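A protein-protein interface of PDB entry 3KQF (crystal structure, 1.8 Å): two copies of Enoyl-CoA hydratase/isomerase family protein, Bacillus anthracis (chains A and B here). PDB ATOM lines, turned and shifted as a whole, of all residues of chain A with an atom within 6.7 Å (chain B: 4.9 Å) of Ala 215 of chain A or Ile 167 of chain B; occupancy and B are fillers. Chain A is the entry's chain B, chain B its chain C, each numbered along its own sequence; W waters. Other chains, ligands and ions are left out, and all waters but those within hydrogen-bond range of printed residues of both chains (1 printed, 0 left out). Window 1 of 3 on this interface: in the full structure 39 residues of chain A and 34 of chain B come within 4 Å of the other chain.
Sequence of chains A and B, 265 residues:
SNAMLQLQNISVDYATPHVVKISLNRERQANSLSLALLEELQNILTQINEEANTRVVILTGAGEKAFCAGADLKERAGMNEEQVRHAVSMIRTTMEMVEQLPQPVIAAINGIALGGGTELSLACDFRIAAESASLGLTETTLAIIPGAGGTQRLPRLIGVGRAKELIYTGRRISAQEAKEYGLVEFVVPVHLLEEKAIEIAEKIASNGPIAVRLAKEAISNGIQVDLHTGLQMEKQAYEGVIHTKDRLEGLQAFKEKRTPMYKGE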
ATOM      1  N   ASN A 207     -24.344 -23.510  14.575  1.00  0.00           N
ATOM      2  CA  ASN A 207     -25.580 -24.187  15.000  1.00  0.00           C
ATOM      3  C   ASN A 207     -26.509 -23.218  15.705  1.00  0.00           C
ATOM      4  O   ASN A 207     -26.110 -22.096  16.029  1.00  0.00           O
ATOM      5  CB  ASN A 207     -25.214 -25.396  15.879  1.00  0.00           C
ATOM      6  CG  ASN A 207     -24.443 -26.458  15.090  1.00  0.00           C
ATOM      7  OD1 ASN A 207     -24.547 -26.519  13.851  1.00  0.00           O
ATOM      8  ND2 ASN A 207     -23.662 -27.276  15.785  1.00  0.00           N
ATOM      9  N   ILE A 210     -29.961 -20.738  20.391  1.00  0.00           N
ATOM     10  CA  ILE A 210     -30.930 -21.063  21.442  1.00  0.00           C
ATOM     11  C   ILE A 210     -30.822 -22.554  21.769  1.00  0.00           C
ATOM     12  O   ILE A 210     -30.847 -22.964  22.930  1.00  0.00           O
ATOM     13  CB  ILE A 210     -32.369 -20.724  21.002  1.00  0.00           C
ATOM     14  CG1 ILE A 210     -32.511 -19.231  20.735  1.00  0.00           C
ATOM     15  CG2 ILE A 210     -33.380 -21.168  22.073  1.00  0.00           C
ATOM     16  CD1 ILE A 210     -33.848 -18.856  20.041  1.00  0.00           C
ATOM     17  N   ALA A 211     -30.705 -23.372  20.729  1.00  0.00           N
ATOM     18  CA  ALA A 211     -30.615 -24.815  20.898  1.00  0.00           C
ATOM     19  C   ALA A 211     -29.318 -25.224  21.628  1.00  0.00           C
ATOM     20  O   ALA A 211     -29.352 -26.049  22.545  1.00  0.00           O
ATOM     21  CB  ALA A 211     -30.740 -25.509  19.543  1.00  0.00           C
ATOM     22  N   VAL A 212     -28.184 -24.647  21.241  1.00  0.00           N
ATOM     23  CA  VAL A 212     -26.911 -24.972  21.919  1.00  0.00           C
ATOM     24  C   VAL A 212     -26.980 -24.577  23.384  1.00  0.00           C
ATOM     25  O   VAL A 212     -26.588 -25.348  24.270  1.00  0.00           O
ATOM     26  CB  VAL A 212     -25.694 -24.306  21.243  1.00  0.00           C
ATOM     27  CG1 VAL A 212     -24.426 -24.492  22.096  1.00  0.00           C
ATOM     28  CG2 VAL A 212     -25.485 -24.927  19.837  1.00  0.00           C
ATOM     29  N   ARG A 213     -27.538 -23.405  23.661  1.00  0.00           N
ATOM     30  CA  ARG A 213     -27.642 -22.951  25.056  1.00  0.00           C
ATOM     31  C   ARG A 213     -28.543 -23.874  25.881  1.00  0.00           C
ATOM     32  O   ARG A 213     -28.178 -24.268  26.993  1.00  0.00           O
ATOM     33  CB  ARG A 213     -28.110 -21.516  25.138  1.00  0.00           C
ATOM     34  CG  ARG A 213     -27.103 -20.520  24.581  1.00  0.00           C
ATOM     35  CD  ARG A 213     -27.609 -19.122  24.830  1.00  0.00           C
ATOM     36  NE  ARG A 213     -26.671 -18.119  24.357  1.00  0.00           N
ATOM     37  CZ  ARG A 213     -26.643 -16.869  24.794  1.00  0.00           C
ATOM     38  NH1 ARG A 213     -27.490 -16.476  25.747  1.00  0.00           N
ATOM     39  NH2 ARG A 213     -25.734 -16.021  24.313  1.00  0.00           N
ATOM     40  N   LEU A 214     -29.692 -24.228  25.326  1.00  0.00           N
ATOM     41  CA  LEU A 214     -30.625 -25.152  26.004  1.00  0.00           C
ATOM     42  C   LEU A 214     -30.004 -26.545  26.167  1.00  0.00           C
ATOM     43  O   LEU A 214     -30.242 -27.221  27.174  1.00  0.00           O
ATOM     44  CB  LEU A 214     -31.947 -25.251  25.255  1.00  0.00           C
ATOM     45  CG  LEU A 214     -32.894 -24.065  25.357  1.00  0.00           C
ATOM     46  CD1 LEU A 214     -34.013 -24.170  24.342  1.00  0.00           C
ATOM     47  CD2 LEU A 214     -33.449 -23.925  26.772  1.00  0.00           C
ATOM     48  N   ALA A 215     -29.199 -26.965  25.192  1.00  0.00           N
ATOM     49  CA  ALA A 215     -28.535 -28.267  25.287  1.00  0.00           C
ATOM     50  C   ALA A 215     -27.573 -28.262  26.460  1.00  0.00           C
ATOM     51  O   ALA A 215     -27.502 -29.258  27.195  1.00  0.00           O
ATOM     52  CB  ALA A 215     -27.818 -28.649  23.972  1.00  0.00           C
ATOM     53  N   LYS A 216     -26.818 -27.160  26.634  1.00  0.00           N
ATOM     54  CA  LYS A 216     -25.868 -27.045  27.742  1.00  0.00           C
ATOM     55  C   LYS A 216     -26.589 -27.131  29.099  1.00  0.00           C
ATOM     56  O   LYS A 216     -26.122 -27.804  30.022  1.00  0.00           O
ATOM     57  CB  LYS A 216     -25.062 -25.749  27.658  1.00  0.00           C
ATOM     58  CG  LYS A 216     -24.202 -25.501  28.894  1.00  0.00           C
ATOM     59  CD  LYS A 216     -23.092 -24.503  28.668  1.00  0.00           C
ATOM     60  CE  LYS A 216     -22.319 -24.275  29.956  1.00  0.00           C
ATOM     61  NZ  LYS A 216     -21.048 -23.530  29.809  1.00  0.00           N
ATOM     62  N   GLU A 217     -27.717 -26.440  29.223  1.00  0.00           N
ATOM     63  CA  GLU A 217     -28.475 -26.481  30.476  1.00  0.00           C
ATOM     64  C   GLU A 217     -29.029 -27.875  30.736  1.00  0.00           C
ATOM     65  O   GLU A 217     -28.886 -28.411  31.851  1.00  0.00           O
ATOM     66  CB  GLU A 217     -29.613 -25.469  30.479  1.00  0.00           C
ATOM     67  CG  GLU A 217     -29.179 -24.031  30.562  1.00  0.00           C
ATOM     68  CD  GLU A 217     -30.368 -23.099  30.672  1.00  0.00           C
ATOM     69  OE1 GLU A 217     -31.419 -23.385  30.047  1.00  0.00           O
ATOM     70  OE2 GLU A 217     -30.252 -22.088  31.383  1.00  0.00           O
ATOM     71  N   ALA A 218     -29.634 -28.479  29.713  1.00  0.00           N
ATOM     72  CA  ALA A 218     -30.220 -29.822  29.872  1.00  0.00           C
ATOM     73  C   ALA A 218     -29.189 -30.861  30.292  1.00  0.00           C
ATOM     74  O   ALA A 218     -29.414 -31.634  31.202  1.00  0.00           O
ATOM     75  CB  ALA A 218     -30.914 -30.285  28.564  1.00  0.00           C
ATOM     76  N   ILE A 219     -28.054 -30.883  29.611  1.00  0.00           N
ATOM     77  CA  ILE A 219     -26.996 -31.805  29.977  1.00  0.00           C
ATOM     78  C   ILE A 219     -26.410 -31.513  31.381  1.00  0.00           C
ATOM     79  O   ILE A 219     -26.283 -32.422  32.217  1.00  0.00           O
ATOM     80  CB  ILE A 219     -25.844 -31.734  28.964  1.00  0.00           C
ATOM     81  CG1 ILE A 219     -26.306 -32.182  27.584  1.00  0.00           C
ATOM     82  CG2 ILE A 219     -24.658 -32.613  29.452  1.00  0.00           C
ATOM     83  CD1 ILE A 219     -25.319 -31.845  26.442  1.00  0.00           C
ATOM     84  N   SER A 220     -26.014 -30.270  31.614  1.00  0.00           N
ATOM     85  CA  SER A 220     -25.310 -29.889  32.846  1.00  0.00           C
ATOM     86  C   SER A 220     -26.138 -30.072  34.102  1.00  0.00           C
ATOM     87  O   SER A 220     -25.614 -30.422  35.169  1.00  0.00           O
ATOM     88  CB  SER A 220     -24.787 -28.446  32.739  1.00  0.00           C
ATOM     89  OG  SER A 220     -23.864 -28.311  31.661  1.00  0.00           O
ATOM     90  N   ALA A 237     -36.788 -28.214  28.242  1.00  0.00           N
ATOM     91  CA  ALA A 237     -35.830 -27.541  27.409  1.00  0.00           C
ATOM     92  C   ALA A 237     -36.277 -27.583  25.924  1.00  0.00           C
ATOM     93  O   ALA A 237     -36.170 -26.586  25.216  1.00  0.00           O
ATOM     94  CB  ALA A 237     -34.429 -28.161  27.599  1.00  0.00           C
ATOM     95  N   LEU B 137     -25.678 -36.998  17.156  1.00  0.00           N
ATOM     96  CA  LEU B 137     -26.891 -36.290  17.558  1.00  0.00           C
ATOM     97  C   LEU B 137     -26.775 -34.951  16.830  1.00  0.00           C
ATOM     98  O   LEU B 137     -26.185 -33.999  17.331  1.00  0.00           O
ATOM     99  CB  LEU B 137     -26.970 -36.122  19.066  1.00  0.00           C
ATOM    100  CG  LEU B 137     -27.268 -37.371  19.901  1.00  0.00           C
ATOM    101  CD1 LEU B 137     -27.259 -37.058  21.404  1.00  0.00           C
ATOM    102  CD2 LEU B 137     -28.622 -37.952  19.479  1.00  0.00           C
ATOM    103  N   THR B 140     -28.617 -29.949  16.996  1.00  0.00           N
ATOM    104  CA  THR B 140     -28.256 -28.522  17.054  1.00  0.00           C
ATOM    105  C   THR B 140     -27.983 -27.876  15.688  1.00  0.00           C
ATOM    106  O   THR B 140     -28.154 -26.652  15.543  1.00  0.00           O
ATOM    107  CB  THR B 140     -27.110 -28.230  18.008  1.00  0.00           C
ATOM    108  OG1 THR B 140     -25.936 -28.939  17.590  1.00  0.00           O
ATOM    109  CG2 THR B 140     -27.501 -28.593  19.455  1.00  0.00           C
ATOM    110  N   ILE B 145     -32.890 -29.564  19.786  1.00  0.00           N
ATOM    111  CA  ILE B 145     -32.050 -30.370  20.667  1.00  0.00           C
ATOM    112  C   ILE B 145     -32.537 -31.810  20.656  1.00  0.00           C
ATOM    113  O   ILE B 145     -33.659 -32.084  20.213  1.00  0.00           O
ATOM    114  CB  ILE B 145     -32.025 -29.859  22.147  1.00  0.00           C
ATOM    115  CG1 ILE B 145     -33.416 -29.949  22.783  1.00  0.00           C
ATOM    116  CG2 ILE B 145     -31.490 -28.421  22.231  1.00  0.00           C
ATOM    117  CD1 ILE B 145     -33.443 -29.499  24.257  1.00  0.00           C
ATOM    118  N   PRO B 146     -31.688 -32.751  21.113  1.00  0.00           N
ATOM    119  CA  PRO B 146     -32.213 -34.091  21.233  1.00  0.00           C
ATOM    120  C   PRO B 146     -33.409 -34.034  22.214  1.00  0.00           C
ATOM    121  O   PRO B 146     -33.284 -33.515  23.320  1.00  0.00           O
ATOM    122  CB  PRO B 146     -31.035 -34.891  21.794  1.00  0.00           C
ATOM    123  CG  PRO B 146     -29.834 -34.129  21.395  1.00  0.00           C
ATOM    124  CD  PRO B 146     -30.247 -32.685  21.418  1.00  0.00           C
ATOM    125  N   GLY B 150     -31.576 -38.026  24.274  1.00  0.00           N
ATOM    126  CA  GLY B 150     -30.199 -37.820  23.856  1.00  0.00           C
ATOM    127  C   GLY B 150     -29.348 -36.988  24.820  1.00  0.00           C
ATOM    128  O   GLY B 150     -28.177 -37.323  25.059  1.00  0.00           O
ATOM    129  N   THR B 151     -29.915 -35.913  25.383  1.00  0.00           N
ATOM    130  CA  THR B 151     -29.153 -35.058  26.323  1.00  0.00           C
ATOM    131  C   THR B 151     -28.903 -35.710  27.675  1.00  0.00           C
ATOM    132  O   THR B 151     -28.078 -35.222  28.449  1.00  0.00           O
ATOM    133  CB  THR B 151     -29.825 -33.704  26.599  1.00  0.00           C
ATOM    134  OG1 THR B 151     -31.110 -33.882  27.257  1.00  0.00           O
ATOM    135  CG2 THR B 151     -30.034 -32.933  25.293  1.00  0.00           C
ATOM    136  N   LEU B 154     -26.949 -39.932  26.688  1.00  0.00           N
ATOM    137  CA  LEU B 154     -25.584 -39.861  26.138  1.00  0.00           C
ATOM    138  C   LEU B 154     -24.529 -39.552  27.237  1.00  0.00           C
ATOM    139  O   LEU B 154     -23.536 -40.284  27.366  1.00  0.00           O
ATOM    140  CB  LEU B 154     -25.485 -38.869  24.971  1.00  0.00           C
ATOM    141  CG  LEU B 154     -24.127 -38.869  24.240  1.00  0.00           C
ATOM    142  CD1 LEU B 154     -23.928 -40.211  23.507  1.00  0.00           C
ATOM    143  CD2 LEU B 154     -24.012 -37.753  23.216  1.00  0.00           C
ATOM    144  N   ALA B 163     -20.129 -36.067  25.598  1.00  0.00           N
ATOM    145  CA  ALA B 163     -21.523 -35.826  25.250  1.00  0.00           C
ATOM    146  C   ALA B 163     -21.723 -34.382  24.806  1.00  0.00           C
ATOM    147  O   ALA B 163     -22.384 -34.131  23.809  1.00  0.00           O
ATOM    148  CB  ALA B 163     -22.432 -36.156  26.412  1.00  0.00           C
ATOM    149  N   LYS B 164     -21.121 -33.439  25.541  1.00  0.00           N
ATOM    150  CA  LYS B 164     -21.213 -32.027  25.183  1.00  0.00           C
ATOM    151  C   LYS B 164     -20.586 -31.705  23.812  1.00  0.00           C
ATOM    152  O   LYS B 164     -21.221 -31.053  22.956  1.00  0.00           O
ATOM    153  CB  LYS B 164     -20.594 -31.167  26.290  1.00  0.00           C
ATOM    154  CG  LYS B 164     -21.482 -31.037  27.514  1.00  0.00           C
ATOM    155  CD  LYS B 164     -20.820 -30.248  28.617  1.00  0.00           C
ATOM    156  CE  LYS B 164     -21.781 -29.877  29.706  1.00  0.00           C
ATOM    157  NZ  LYS B 164     -21.212 -28.871  30.685  1.00  0.00           N
ATOM    158  N   GLU B 165     -19.363 -32.166  23.575  1.00  0.00           N
ATOM    159  CA  GLU B 165     -18.748 -31.839  22.307  1.00  0.00           C
ATOM    160  C   GLU B 165     -19.583 -32.399  21.171  1.00  0.00           C
ATOM    161  O   GLU B 165     -19.843 -31.687  20.198  1.00  0.00           O
ATOM    162  CB  GLU B 165     -17.262 -32.240  22.227  1.00  0.00           C
ATOM    163  CG  GLU B 165     -16.931 -33.705  22.124  1.00  0.00           C
ATOM    164  CD  GLU B 165     -16.842 -34.255  20.675  1.00  0.00           C
ATOM    165  OE1 GLU B 165     -16.336 -35.388  20.550  1.00  0.00           O
ATOM    166  OE2 GLU B 165     -17.226 -33.580  19.681  1.00  0.00           O
ATOM    167  N   LEU B 166     -20.103 -33.616  21.341  1.00  0.00           N
ATOM    168  CA  LEU B 166     -20.939 -34.256  20.299  1.00  0.00           C
ATOM    169  C   LEU B 166     -22.292 -33.558  20.039  1.00  0.00           C
ATOM    170  O   LEU B 166     -22.693 -33.361  18.878  1.00  0.00           O
ATOM    171  CB  LEU B 166     -21.178 -35.719  20.642  1.00  0.00           C
ATOM    172  CG  LEU B 166     -19.973 -36.662  20.528  1.00  0.00           C
ATOM    173  CD1 LEU B 166     -20.387 -38.061  20.993  1.00  0.00           C
ATOM    174  CD2 LEU B 166     -19.454 -36.685  19.103  1.00  0.00           C
ATOM    175  N   ILE B 167     -22.972 -33.182  21.117  1.00  0.00           N
ATOM    176  CA  ILE B 167     -24.262 -32.488  21.027  1.00  0.00           C
ATOM    177  C   ILE B 167     -24.094 -31.029  20.575  1.00  0.00           C
ATOM    178  O   ILE B 167     -24.849 -30.561  19.708  1.00  0.00           O
ATOM    179  CB  ILE B 167     -25.038 -32.597  22.342  1.00  0.00           C
ATOM    180  CG1 ILE B 167     -25.450 -34.062  22.534  1.00  0.00           C
ATOM    181  CG2 ILE B 167     -26.279 -31.654  22.348  1.00  0.00           C
ATOM    182  CD1 ILE B 167     -26.033 -34.393  23.879  1.00  0.00           C
ATOM    183  N   TYR B 168     -23.082 -30.327  21.100  1.00  0.00           N
ATOM    184  CA  TYR B 168     -22.871 -28.929  20.679  1.00  0.00           C
ATOM    185  C   TYR B 168     -22.473 -28.822  19.210  1.00  0.00           C
ATOM    186  O   TYR B 168     -22.985 -27.949  18.497  1.00  0.00           O
ATOM    187  CB  TYR B 168     -21.827 -28.200  21.518  1.00  0.00           C
ATOM    188  CG  TYR B 168     -22.077 -28.121  23.015  1.00  0.00           C
ATOM    189  CD1 TYR B 168     -23.359 -28.228  23.559  1.00  0.00           C
ATOM    190  CD2 TYR B 168     -21.038 -27.792  23.863  1.00  0.00           C
ATOM    191  CE1 TYR B 168     -23.563 -28.145  24.925  1.00  0.00           C
ATOM    192  CE2 TYR B 168     -21.238 -27.678  25.227  1.00  0.00           C
ATOM    193  CZ  TYR B 168     -22.491 -27.846  25.754  1.00  0.00           C
ATOM    194  OH  TYR B 168     -22.660 -27.723  27.106  1.00  0.00           O
ATOM    195  N   THR B 169     -21.535 -29.663  18.763  1.00  0.00           N
ATOM    196  CA  THR B 169     -21.120 -29.656  17.360  1.00  0.00           C
ATOM    197  C   THR B 169     -22.127 -30.286  16.411  1.00  0.00           C
ATOM    198  O   THR B 169     -22.206 -29.885  15.243  1.00  0.00           O
ATOM    199  CB  THR B 169     -19.786 -30.384  17.118  1.00  0.00           C
ATOM    200  OG1 THR B 169     -19.913 -31.778  17.433  1.00  0.00           O
ATOM    201  CG2 THR B 169     -18.651 -29.747  17.956  1.00  0.00           C
ATOM    202  N   GLY B 170     -22.869 -31.281  16.904  1.00  0.00           N
ATOM    203  CA  GLY B 170     -23.842 -32.018  16.099  1.00  0.00           C
ATOM    204  C   GLY B 170     -23.152 -32.846  15.039  1.00  0.00           C
ATOM    205  O   GLY B 170     -23.762 -33.212  14.029  1.00  0.00           O
HETATM  206  O   HOH W   1     -21.490 -26.996  32.717  1.00  0.00           O
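The side-chain amide nitrogen (ND2) of Asn 207 of chain A lies within hydrogen-bond range of the backbone carbonyl oxygen (O) of Thr 169 of chain B, at 3.0 Å.
The side-chain hydroxyl of Ser 220 of chain A lies within hydrogen-bond range of the side-chain amino group of Lys 164 of chain B, 2.9 Å away.
The side-chain amide nitrogen (ND2) of Asn 207 of chain A lies within hydrogen-bond range of the backbone carbonyl oxygen (O) of Tyr 168 of chain B, 2.9 Å away.
OG1 of Thr 140 of chain B lies within hydrogen-bond range of ND2 of Asn 207 of chain A (3.3 Å).
The side-chain hydroxyl (OG1) of Thr 140 of chain B is in hydrogen-bond range of the backbone carbonyl oxygen (O) of Tyr 168 of chain B (3.2 Å).
The side-chain hydroxyl of Thr 140 of chain B sits at hydrogen-bond distance from the backbone carbonyl oxygen of Ile 167 of chain B.
The side-chain hydroxyl of Thr 169 of chain B sits at hydrogen-bond distance from the backbone carbonyl oxygen of Glu 165 of chain B, 2.8 Å away.
O of Lys 216 of chain A lies within hydrogen-bond range of OG of Ser 220 of chain A (2.8 Å).
Among the printed residues, merely in contact across the chains: Lys 216 of chain A with Tyr 168 of chain B (3.2 Å), Ala 211 of chain A with Ile 145 of chain B (3.2 Å), Ile 219 of chain A with Thr 151 of chain B (3.6 Å), Ile 219 of chain A with Ile 167 of chain B (3.7 Å), Ala 237 of chain A with Ile 145 of chain B (3.7 Å), Ala 215 of chain A with Ile 167 of chain B (3.7 Å), Ala 218 of chain A with Thr 151 of chain B (3.8 Å) and Ile 219 of chain A with Lys 164 of chain B (3.98 Å).
Ile 167 of chain B touches just these residues of chain A: Ala 215 and Ile 219.
Printed residues of chain B within 4 Å of Ile 219 of chain A: Thr 151, Lys 164 and Ile 167.
Printed residues of chain A within 4 Å of Ile 145 of chain B: Ala 211 and Ala 237.
Of the printed residues of chain B, Ala 237 of chain A touches Ile 145.
Printed residues of chain A within 4 Å of Thr 169 of chain B: Asn 207.
Printed residues of chain A within 4 Å of Lys 164 of chain B: Ile 219 and Ser 220.
Ala 163 of chain B touches none of the printed residues of chain A.
Arg 213 of chain A touches none of the printed residues of chain B.
The nearest printed residue of chain B that does not touch Ala 215 of chain A is Ile 145 of chain B (4.02 Å).
The nearest printed residue of chain B that does not touch Asn 207 of chain A is Gly 170 of chain B (4.2 Å).
Hydrophobic or aromatic side chains of chain B that line the printed part of chain A: Ile 145, Ile 167 and Tyr 168.
Hydrophobic or aromatic side chains of chain A within 4 Å of the printed part of chain B: Ala 215, Ala 218, Ile 219 and Ala 237.
Among the printed residues, 12 pairs touch across the chains.
No position is printed for both chains.
Of the 12 pairs that touch across the chains among the printed residues, none has its exchanged pair printed and touching as well.
Water W1 lies within hydrogen-bond range of the side-chain amino group (NZ) of Lys 164 of chain B (2.8 Å) and the side-chain hydroxyl (OG) of Ser 220 of chain A (2.9 Å).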
